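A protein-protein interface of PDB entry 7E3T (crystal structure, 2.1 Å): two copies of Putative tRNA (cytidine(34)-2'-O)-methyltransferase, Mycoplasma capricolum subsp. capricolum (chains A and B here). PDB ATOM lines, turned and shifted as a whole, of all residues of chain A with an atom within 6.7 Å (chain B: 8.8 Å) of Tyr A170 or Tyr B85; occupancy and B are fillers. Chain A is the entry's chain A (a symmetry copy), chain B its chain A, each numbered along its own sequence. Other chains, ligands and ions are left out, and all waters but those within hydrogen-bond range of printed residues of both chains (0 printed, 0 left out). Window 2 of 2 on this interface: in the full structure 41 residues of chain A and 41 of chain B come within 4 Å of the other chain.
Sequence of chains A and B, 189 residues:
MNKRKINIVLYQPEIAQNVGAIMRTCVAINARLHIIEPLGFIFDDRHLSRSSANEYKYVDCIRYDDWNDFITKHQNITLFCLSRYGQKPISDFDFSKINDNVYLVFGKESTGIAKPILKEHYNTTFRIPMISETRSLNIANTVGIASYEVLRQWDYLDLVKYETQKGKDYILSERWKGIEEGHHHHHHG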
ATOM      1  N   GLU A 163      21.113  15.983 -27.137  1.00  0.00           N
ATOM      2  CA  GLU A 163      21.202  14.754 -27.966  1.00  0.00           C
ATOM      3  C   GLU A 163      21.028  15.179 -29.413  1.00  0.00           C
ATOM      4  O   GLU A 163      20.131  15.997 -29.675  1.00  0.00           O
ATOM      5  CB  GLU A 163      20.128  13.710 -27.636  1.00  0.00           C
ATOM      6  N   THR A 164      21.831  14.599 -30.300  1.00  0.00           N
ATOM      7  CA  THR A 164      21.669  14.682 -31.776  1.00  0.00           C
ATOM      8  C   THR A 164      20.421  13.882 -32.187  1.00  0.00           C
ATOM      9  O   THR A 164      19.873  13.151 -31.336  1.00  0.00           O
ATOM     10  CB  THR A 164      22.923  14.170 -32.498  1.00  0.00           C
ATOM     11  OG1 THR A 164      22.841  12.742 -32.517  1.00  0.00           O
ATOM     12  CG2 THR A 164      24.215  14.628 -31.848  1.00  0.00           C
ATOM     13  N   GLN A 165      20.000  14.009 -33.448  1.00  0.00           N
ATOM     14  CA  GLN A 165      18.903  13.214 -34.063  1.00  0.00           C
ATOM     15  C   GLN A 165      19.326  11.737 -34.184  1.00  0.00           C
ATOM     16  O   GLN A 165      18.420  10.878 -34.258  1.00  0.00           O
ATOM     17  CB  GLN A 165      18.533  13.830 -35.417  1.00  0.00           C
ATOM     18  CG  GLN A 165      17.259  13.273 -36.037  1.00  0.00           C
ATOM     19  CD  GLN A 165      16.160  13.114 -35.017  1.00  0.00           C
ATOM     20  OE1 GLN A 165      15.455  14.064 -34.686  1.00  0.00           O
ATOM     21  NE2 GLN A 165      16.022  11.906 -34.494  1.00  0.00           N
ATOM     22  N   LYS A 166      20.637  11.448 -34.203  1.00  0.00           N
ATOM     23  CA  LYS A 166      21.216  10.073 -34.160  1.00  0.00           C
ATOM     24  C   LYS A 166      20.726   9.350 -32.897  1.00  0.00           C
ATOM     25  O   LYS A 166      20.223   8.197 -33.018  1.00  0.00           O
ATOM     26  CB  LYS A 166      22.750  10.117 -34.182  1.00  0.00           C
ATOM     27  N   GLY A 167      20.861  10.010 -31.738  1.00  0.00           N
ATOM     28  CA  GLY A 167      20.465   9.485 -30.417  1.00  0.00           C
ATOM     29  C   GLY A 167      18.967   9.242 -30.320  1.00  0.00           C
ATOM     30  O   GLY A 167      18.580   8.124 -29.953  1.00  0.00           O
ATOM     31  N   LYS A 168      18.149  10.246 -30.652  1.00  0.00           N
ATOM     32  CA  LYS A 168      16.682  10.279 -30.379  1.00  0.00           C
ATOM     33  C   LYS A 168      15.961   9.183 -31.184  1.00  0.00           C
ATOM     34  O   LYS A 168      15.183   8.425 -30.563  1.00  0.00           O
ATOM     35  CB  LYS A 168      16.112  11.675 -30.670  1.00  0.00           C
ATOM     36  N   ASP A 169      16.199   9.110 -32.504  1.00  0.00           N
ATOM     37  CA  ASP A 169      15.509   8.177 -33.442  1.00  0.00           C
ATOM     38  C   ASP A 169      16.187   6.805 -33.361  1.00  0.00           C
ATOM     39  O   ASP A 169      15.685   5.855 -34.007  1.00  0.00           O
ATOM     40  CB  ASP A 169      15.482   8.708 -34.880  1.00  0.00           C
ATOM     41  N   TYR A 170      17.293   6.712 -32.615  1.00  0.00           N
ATOM     42  CA  TYR A 170      17.868   5.421 -32.164  1.00  0.00           C
ATOM     43  C   TYR A 170      16.927   4.819 -31.101  1.00  0.00           C
ATOM     44  O   TYR A 170      16.459   3.671 -31.300  1.00  0.00           O
ATOM     45  CB  TYR A 170      19.314   5.600 -31.695  1.00  0.00           C
ATOM     46  CG  TYR A 170      19.845   4.419 -30.929  1.00  0.00           C
ATOM     47  CD1 TYR A 170      19.521   3.130 -31.325  1.00  0.00           C
ATOM     48  CD2 TYR A 170      20.649   4.574 -29.813  1.00  0.00           C
ATOM     49  CE1 TYR A 170      19.979   2.021 -30.637  1.00  0.00           C
ATOM     50  CE2 TYR A 170      21.122   3.474 -29.115  1.00  0.00           C
ATOM     51  CZ  TYR A 170      20.785   2.197 -29.531  1.00  0.00           C
ATOM     52  OH  TYR A 170      21.239   1.096 -28.874  1.00  0.00           O
ATOM     53  N   ILE A 171      16.627   5.582 -30.037  1.00  0.00           N
ATOM     54  CA  ILE A 171      15.824   5.150 -28.847  1.00  0.00           C
ATOM     55  C   ILE A 171      14.329   5.101 -29.217  1.00  0.00           C
ATOM     56  O   ILE A 171      13.683   4.090 -28.880  1.00  0.00           O
ATOM     57  CB  ILE A 171      16.112   6.059 -27.620  1.00  0.00           C
ATOM     58  CG1 ILE A 171      17.365   5.611 -26.862  1.00  0.00           C
ATOM     59  CG2 ILE A 171      14.915   6.163 -26.678  1.00  0.00           C
ATOM     60  CD1 ILE A 171      18.186   6.756 -26.322  1.00  0.00           C
ATOM     61  N   LEU A 172      13.784   6.145 -29.858  1.00  0.00           N
ATOM     62  CA  LEU A 172      12.338   6.223 -30.225  1.00  0.00           C
ATOM     63  C   LEU A 172      12.025   5.197 -31.332  1.00  0.00           C
ATOM     64  O   LEU A 172      10.840   5.117 -31.710  1.00  0.00           O
ATOM     65  CB  LEU A 172      11.973   7.650 -30.653  1.00  0.00           C
ATOM     66  N   SER A 173      13.034   4.442 -31.812  1.00  0.00           N
ATOM     67  CA  SER A 173      12.907   3.309 -32.773  1.00  0.00           C
ATOM     68  C   SER A 173      13.800   2.126 -32.353  1.00  0.00           C
ATOM     69  O   SER A 173      13.337   1.322 -31.517  1.00  0.00           O
ATOM     70  CB  SER A 173      13.197   3.754 -34.189  1.00  0.00           C
ATOM     71  OG  SER A 173      12.185   4.633 -34.654  1.00  0.00           O
ATOM     72  N   GLU A 174      15.028   2.030 -32.896  1.00  0.00           N
ATOM     73  CA  GLU A 174      15.859   0.787 -32.943  1.00  0.00           C
ATOM     74  C   GLU A 174      15.696  -0.019 -31.648  1.00  0.00           C
ATOM     75  O   GLU A 174      14.759  -0.828 -31.594  1.00  0.00           O
ATOM     76  CB  GLU A 174      17.334   1.107 -33.204  1.00  0.00           C
ATOM     77  N   CYS B  81      14.589  10.557 -16.107  1.00  0.00           N
ATOM     78  CA  CYS B  81      15.622   9.500 -16.215  1.00  0.00           C
ATOM     79  C   CYS B  81      16.940  10.098 -16.725  1.00  0.00           C
ATOM     80  O   CYS B  81      16.938  10.773 -17.777  1.00  0.00           O
ATOM     81  CB  CYS B  81      15.177   8.393 -17.163  1.00  0.00           C
ATOM     82  SG  CYS B  81      13.730   7.452 -16.599  1.00  0.00           S
ATOM     83  N   LEU B  82      18.030   9.828 -16.017  1.00  0.00           N
ATOM     84  CA  LEU B  82      19.389  10.199 -16.470  1.00  0.00           C
ATOM     85  C   LEU B  82      19.799   9.212 -17.568  1.00  0.00           C
ATOM     86  O   LEU B  82      19.747   7.975 -17.323  1.00  0.00           O
ATOM     87  CB  LEU B  82      20.407  10.140 -15.327  1.00  0.00           C
ATOM     88  CG  LEU B  82      21.868  10.372 -15.757  1.00  0.00           C
ATOM     89  CD1 LEU B  82      22.077  11.770 -16.293  1.00  0.00           C
ATOM     90  CD2 LEU B  82      22.825  10.117 -14.604  1.00  0.00           C
ATOM     91  N   SER B  83      20.266   9.754 -18.692  1.00  0.00           N
ATOM     92  CA  SER B  83      20.884   8.988 -19.791  1.00  0.00           C
ATOM     93  C   SER B  83      22.004   9.793 -20.454  1.00  0.00           C
ATOM     94  O   SER B  83      21.842  11.014 -20.590  1.00  0.00           O
ATOM     95  CB  SER B  83      19.823   8.596 -20.782  1.00  0.00           C
ATOM     96  OG  SER B  83      20.371   7.771 -21.793  1.00  0.00           O
ATOM     97  N   ARG B  84      23.077   9.103 -20.873  1.00  0.00           N
ATOM     98  CA  ARG B  84      24.061   9.572 -21.893  1.00  0.00           C
ATOM     99  C   ARG B  84      23.309  10.182 -23.092  1.00  0.00           C
ATOM    100  O   ARG B  84      23.747  11.226 -23.583  1.00  0.00           O
ATOM    101  CB  ARG B  84      24.994   8.422 -22.312  1.00  0.00           C
ATOM    102  N   TYR B  85      22.173   9.596 -23.491  1.00  0.00           N
ATOM    103  CA  TYR B  85      21.393   9.982 -24.697  1.00  0.00           C
ATOM    104  C   TYR B  85      20.188  10.867 -24.330  1.00  0.00           C
ATOM    105  O   TYR B  85      19.299  11.024 -25.168  1.00  0.00           O
ATOM    106  CB  TYR B  85      20.992   8.714 -25.460  1.00  0.00           C
ATOM    107  CG  TYR B  85      22.141   7.855 -25.938  1.00  0.00           C
ATOM    108  CD1 TYR B  85      23.471   8.243 -25.770  1.00  0.00           C
ATOM    109  CD2 TYR B  85      21.900   6.662 -26.604  1.00  0.00           C
ATOM    110  CE1 TYR B  85      24.525   7.456 -26.213  1.00  0.00           C
ATOM    111  CE2 TYR B  85      22.942   5.868 -27.061  1.00  0.00           C
ATOM    112  CZ  TYR B  85      24.258   6.263 -26.864  1.00  0.00           C
ATOM    113  OH  TYR B  85      25.284   5.481 -27.315  1.00  0.00           O
ATOM    114  N   GLY B  86      20.172  11.465 -23.134  1.00  0.00           N
ATOM    115  CA  GLY B  86      19.092  12.358 -22.670  1.00  0.00           C
ATOM    116  C   GLY B  86      19.050  13.627 -23.496  1.00  0.00           C
ATOM    117  O   GLY B  86      20.110  14.092 -23.962  1.00  0.00           O
ATOM    118  N   GLN B  87      17.852  14.153 -23.714  1.00  0.00           N
ATOM    119  CA  GLN B  87      17.590  15.196 -24.729  1.00  0.00           C
ATOM    120  C   GLN B  87      18.302  16.476 -24.356  1.00  0.00           C
ATOM    121  O   GLN B  87      18.902  17.098 -25.244  1.00  0.00           O
ATOM    122  CB  GLN B  87      16.105  15.483 -24.831  1.00  0.00           C
ATOM    123  CG  GLN B  87      15.346  14.293 -25.374  1.00  0.00           C
ATOM    124  CD  GLN B  87      13.930  14.698 -25.669  1.00  0.00           C
ATOM    125  OE1 GLN B  87      13.654  15.872 -25.916  1.00  0.00           O
ATOM    126  NE2 GLN B  87      13.028  13.734 -25.603  1.00  0.00           N
ATOM    127  N   LYS B  88      18.234  16.856 -23.089  1.00  0.00           N
ATOM    128  CA  LYS B  88      18.761  18.163 -22.650  1.00  0.00           C
ATOM    129  C   LYS B  88      19.147  18.097 -21.187  1.00  0.00           C
ATOM    130  O   LYS B  88      18.749  17.174 -20.469  1.00  0.00           O
ATOM    131  CB  LYS B  88      17.653  19.201 -22.843  1.00  0.00           C
ATOM    132  CG  LYS B  88      16.335  18.870 -22.152  1.00  0.00           C
ATOM    133  CD  LYS B  88      15.262  19.909 -22.411  1.00  0.00           C
ATOM    134  CE  LYS B  88      14.061  19.764 -21.496  1.00  0.00           C
ATOM    135  NZ  LYS B  88      12.950  20.664 -21.894  1.00  0.00           N
ATOM    136  N   LYS B 115      16.767   0.103 -21.810  1.00  0.00           N
ATOM    137  CA  LYS B 115      16.341   0.854 -23.033  1.00  0.00           C
ATOM    138  C   LYS B 115      14.820   0.970 -23.092  1.00  0.00           C
ATOM    139  O   LYS B 115      14.310   2.048 -23.375  1.00  0.00           O
ATOM    140  CB  LYS B 115      16.905   0.216 -24.313  1.00  0.00           C
ATOM    141  N   LEU B 118      13.716   3.997 -20.997  1.00  0.00           N
ATOM    142  CA  LEU B 118      14.103   5.291 -21.612  1.00  0.00           C
ATOM    143  C   LEU B 118      13.124   5.631 -22.752  1.00  0.00           C
ATOM    144  O   LEU B 118      12.545   6.779 -22.740  1.00  0.00           O
ATOM    145  CB  LEU B 118      15.567   5.194 -22.053  1.00  0.00           C
ATOM    146  CG  LEU B 118      16.595   5.068 -20.927  1.00  0.00           C
ATOM    147  CD1 LEU B 118      17.986   4.823 -21.484  1.00  0.00           C
ATOM    148  CD2 LEU B 118      16.607   6.298 -20.038  1.00  0.00           C
ATOM    149  N   LYS B 119      12.888   4.667 -23.653  1.00  0.00           N
ATOM    150  CA  LYS B 119      11.896   4.770 -24.754  1.00  0.00           C
ATOM    151  C   LYS B 119      10.561   5.204 -24.150  1.00  0.00           C
ATOM    152  O   LYS B 119      10.050   6.251 -24.561  1.00  0.00           O
ATOM    153  CB  LYS B 119      11.751   3.437 -25.502  1.00  0.00           C
ATOM    154  N   TYR B 122      11.040   8.874 -22.859  1.00  0.00           N
ATOM    155  CA  TYR B 122      12.024   9.676 -23.618  1.00  0.00           C
ATOM    156  C   TYR B 122      11.804  11.185 -23.406  1.00  0.00           C
ATOM    157  O   TYR B 122      12.821  11.922 -23.393  1.00  0.00           O
ATOM    158  CB  TYR B 122      12.105   9.277 -25.097  1.00  0.00           C
ATOM    159  CG  TYR B 122      13.396   9.803 -25.659  1.00  0.00           C
ATOM    160  CD1 TYR B 122      14.589   9.372 -25.103  1.00  0.00           C
ATOM    161  CD2 TYR B 122      13.442  10.837 -26.577  1.00  0.00           C
ATOM    162  CE1 TYR B 122      15.808   9.883 -25.507  1.00  0.00           C
ATOM    163  CE2 TYR B 122      14.657  11.359 -27.000  1.00  0.00           C
ATOM    164  CZ  TYR B 122      15.846  10.876 -26.465  1.00  0.00           C
ATOM    165  OH  TYR B 122      17.084  11.333 -26.822  1.00  0.00           O
ATOM    166  N   THR B 125      13.747  12.470 -20.190  1.00  0.00           N
ATOM    167  CA  THR B 125      15.150  12.046 -20.023  1.00  0.00           C
ATOM    168  C   THR B 125      16.018  13.293 -20.031  1.00  0.00           C
ATOM    169  O   THR B 125      15.717  14.247 -20.764  1.00  0.00           O
ATOM    170  CB  THR B 125      15.584  11.041 -21.085  1.00  0.00           C
ATOM    171  OG1 THR B 125      15.524  11.713 -22.344  1.00  0.00           O
ATOM    172  CG2 THR B 125      14.720   9.805 -21.033  1.00  0.00           C
ATOM    173  N   PHE B 126      17.020  13.307 -19.167  1.00  0.00           N
ATOM    174  CA  PHE B 126      17.938  14.447 -19.031  1.00  0.00           C
ATOM    175  C   PHE B 126      19.361  13.897 -19.117  1.00  0.00           C
ATOM    176  O   PHE B 126      19.584  12.694 -18.931  1.00  0.00           O
ATOM    177  CB  PHE B 126      17.663  15.209 -17.741  1.00  0.00           C
ATOM    178  CG  PHE B 126      17.973  14.446 -16.469  1.00  0.00           C
ATOM    179  CD1 PHE B 126      16.990  13.722 -15.815  1.00  0.00           C
ATOM    180  CD2 PHE B 126      19.224  14.530 -15.884  1.00  0.00           C
ATOM    181  CE1 PHE B 126      17.264  13.051 -14.628  1.00  0.00           C
ATOM    182  CE2 PHE B 126      19.496  13.875 -14.688  1.00  0.00           C
ATOM    183  CZ  PHE B 126      18.522  13.117 -14.075  1.00  0.00           C
ATOM    184  N   ARG B 127      20.293  14.781 -19.409  1.00  0.00           N
ATOM    185  CA  ARG B 127      21.736  14.435 -19.397  1.00  0.00           C
ATOM    186  C   ARG B 127      22.434  15.422 -18.485  1.00  0.00           C
ATOM    187  O   ARG B 127      21.857  16.479 -18.200  1.00  0.00           O
ATOM    188  CB  ARG B 127      22.332  14.495 -20.810  1.00  0.00           C
ATOM    189  CG  ARG B 127      22.392  15.888 -21.423  1.00  0.00           C
ATOM    190  CD  ARG B 127      23.253  15.901 -22.691  1.00  0.00           C
ATOM    191  NE  ARG B 127      22.664  14.991 -23.655  1.00  0.00           N
ATOM    192  CZ  ARG B 127      23.314  14.313 -24.578  1.00  0.00           C
ATOM    193  NH1 ARG B 127      24.612  14.470 -24.729  1.00  0.00           N
ATOM    194  NH2 ARG B 127      22.656  13.487 -25.364  1.00  0.00           N
ATOM    195  N   ILE B 128      23.646  15.087 -18.079  1.00  0.00           N
ATOM    196  CA  ILE B 128      24.584  16.006 -17.380  1.00  0.00           C
ATOM    197  C   ILE B 128      25.598  16.386 -18.447  1.00  0.00           C
ATOM    198  O   ILE B 128      26.331  15.513 -18.907  1.00  0.00           O
ATOM    199  CB  ILE B 128      25.270  15.321 -16.171  1.00  0.00           C
ATOM    200  CG1 ILE B 128      24.292  14.502 -15.317  1.00  0.00           C
ATOM    201  CG2 ILE B 128      26.051  16.331 -15.339  1.00  0.00           C
ATOM    202  CD1 ILE B 128      23.532  15.290 -14.297  1.00  0.00           C
ATOM    203  N   MET B 130      28.834  17.155 -20.437  1.00  0.00           N
ATOM    204  CA  MET B 130      30.282  16.886 -20.290  1.00  0.00           C
ATOM    205  C   MET B 130      31.000  17.221 -21.605  1.00  0.00           C
ATOM    206  O   MET B 130      30.341  17.374 -22.647  1.00  0.00           O
ATOM    207  CB  MET B 130      30.486  15.408 -19.966  1.00  0.00           C
ATOM    208  CG  MET B 130      29.682  14.953 -18.757  1.00  0.00           C
ATOM    209  SD  MET B 130      30.091  13.270 -18.362  1.00  0.00           S
ATOM    210  CE  MET B 130      29.072  12.475 -19.599  1.00  0.00           C
ATOM    211  N   GLU B 133      31.500  12.191 -25.065  1.00  0.00           N
ATOM    212  CA  GLU B 133      30.797  10.910 -24.811  1.00  0.00           C
ATOM    213  C   GLU B 133      31.771   9.878 -24.250  1.00  0.00           C
ATOM    214  O   GLU B 133      31.314   8.965 -23.601  1.00  0.00           O
ATOM    215  CB  GLU B 133      30.160  10.416 -26.112  1.00  0.00           C
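The backbone NH of Glu A163 lies within hydrogen-bond range of the backbone carbonyl oxygen of Gln B87.
The backbone NH (N) of Glu A163 sits close to the guanidinium group (NH2) of Arg B127 (3.4 Å).
The backbone carbonyl oxygen (O) of Arg B84 sits at hydrogen-bond distance from the guanidinium group (NH2) of Arg B127 (3.1 Å).
The backbone NH (N) of Tyr B85 sits close to the side-chain hydroxyl (OG) of Ser B83, at 3.1 Å.
The backbone carbonyl oxygen (O) of Lys B88 lies within hydrogen-bond range of the backbone NH (N) of Arg B127, 3.0 Å away.
The backbone carbonyl oxygen (O) of Tyr B85 lies within hydrogen-bond range of the side-chain hydroxyl (OH) of Tyr B122.
The backbone carbonyl oxygen (O) of Tyr B122 lies within hydrogen-bond range of the side-chain hydroxyl (OG1) of Thr B125, at 2.9 Å.
O of Gly B86 lies within hydrogen-bond range of NE of Arg B127 (2.7 Å).
CB of Glu A163 touches O of Tyr B85 (3.7 Å).
Gly B86 touches Glu A163 (O to CB, 3.7 Å).
Glu A163 touches Tyr B122 (CB to OH, 3.9 Å).
Tyr B122 touches Lys A168.
Tyr A170 touches Tyr B85.
Ile A171 touches Tyr B85 (CD1 to CB, 3.5 Å).
CG2 of Ile A171 touches CA of Lys B119 (3.8 Å).
Ile A171 touches Tyr B122.
Of chain B, only Tyr B85 comes within 4 Å of Tyr A170.
Of the printed residues of chain A, Tyr B85 touches Glu A163, Tyr A170 and Ile A171.
No residue of chain B comes within 4 Å of Gly A167.
No residue of chain B comes within 4 Å of Asp A169.
Of the printed residues of chain B, Lys A168 touches Tyr B122.
Of the printed residues of chain A, Tyr B122 touches Glu A163, Lys A168 and Ile A171.
Printed residues of chain A within 4 Å of Arg B127: Glu A163 (3.2 Å).
Of the printed residues of chain B, Ile A171 touches Tyr B85 (3.5 Å), Lys B119 (3.8 Å) and Tyr B122 (3.6 Å).
The nearest residue of chain A that does not touch Tyr B85 is Gly A167 (4.9 Å).
Along chain A the printed residues that touch a printed residue of chain B span positions 163 to 171.
Of the 18 printed residues of chain B, 6 touch a printed residue of chain A.
Printed residues of chain B that touch a printed residue of chain A: Tyr B85, Gly B86, Gln B87, Lys B119, Tyr B122 and Arg B127.
Along chain B the printed residues that touch a printed residue of chain A span positions 85 to 127.
Among the printed residues, 10 pairs touch across the chains.
No position is printed for both chains.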
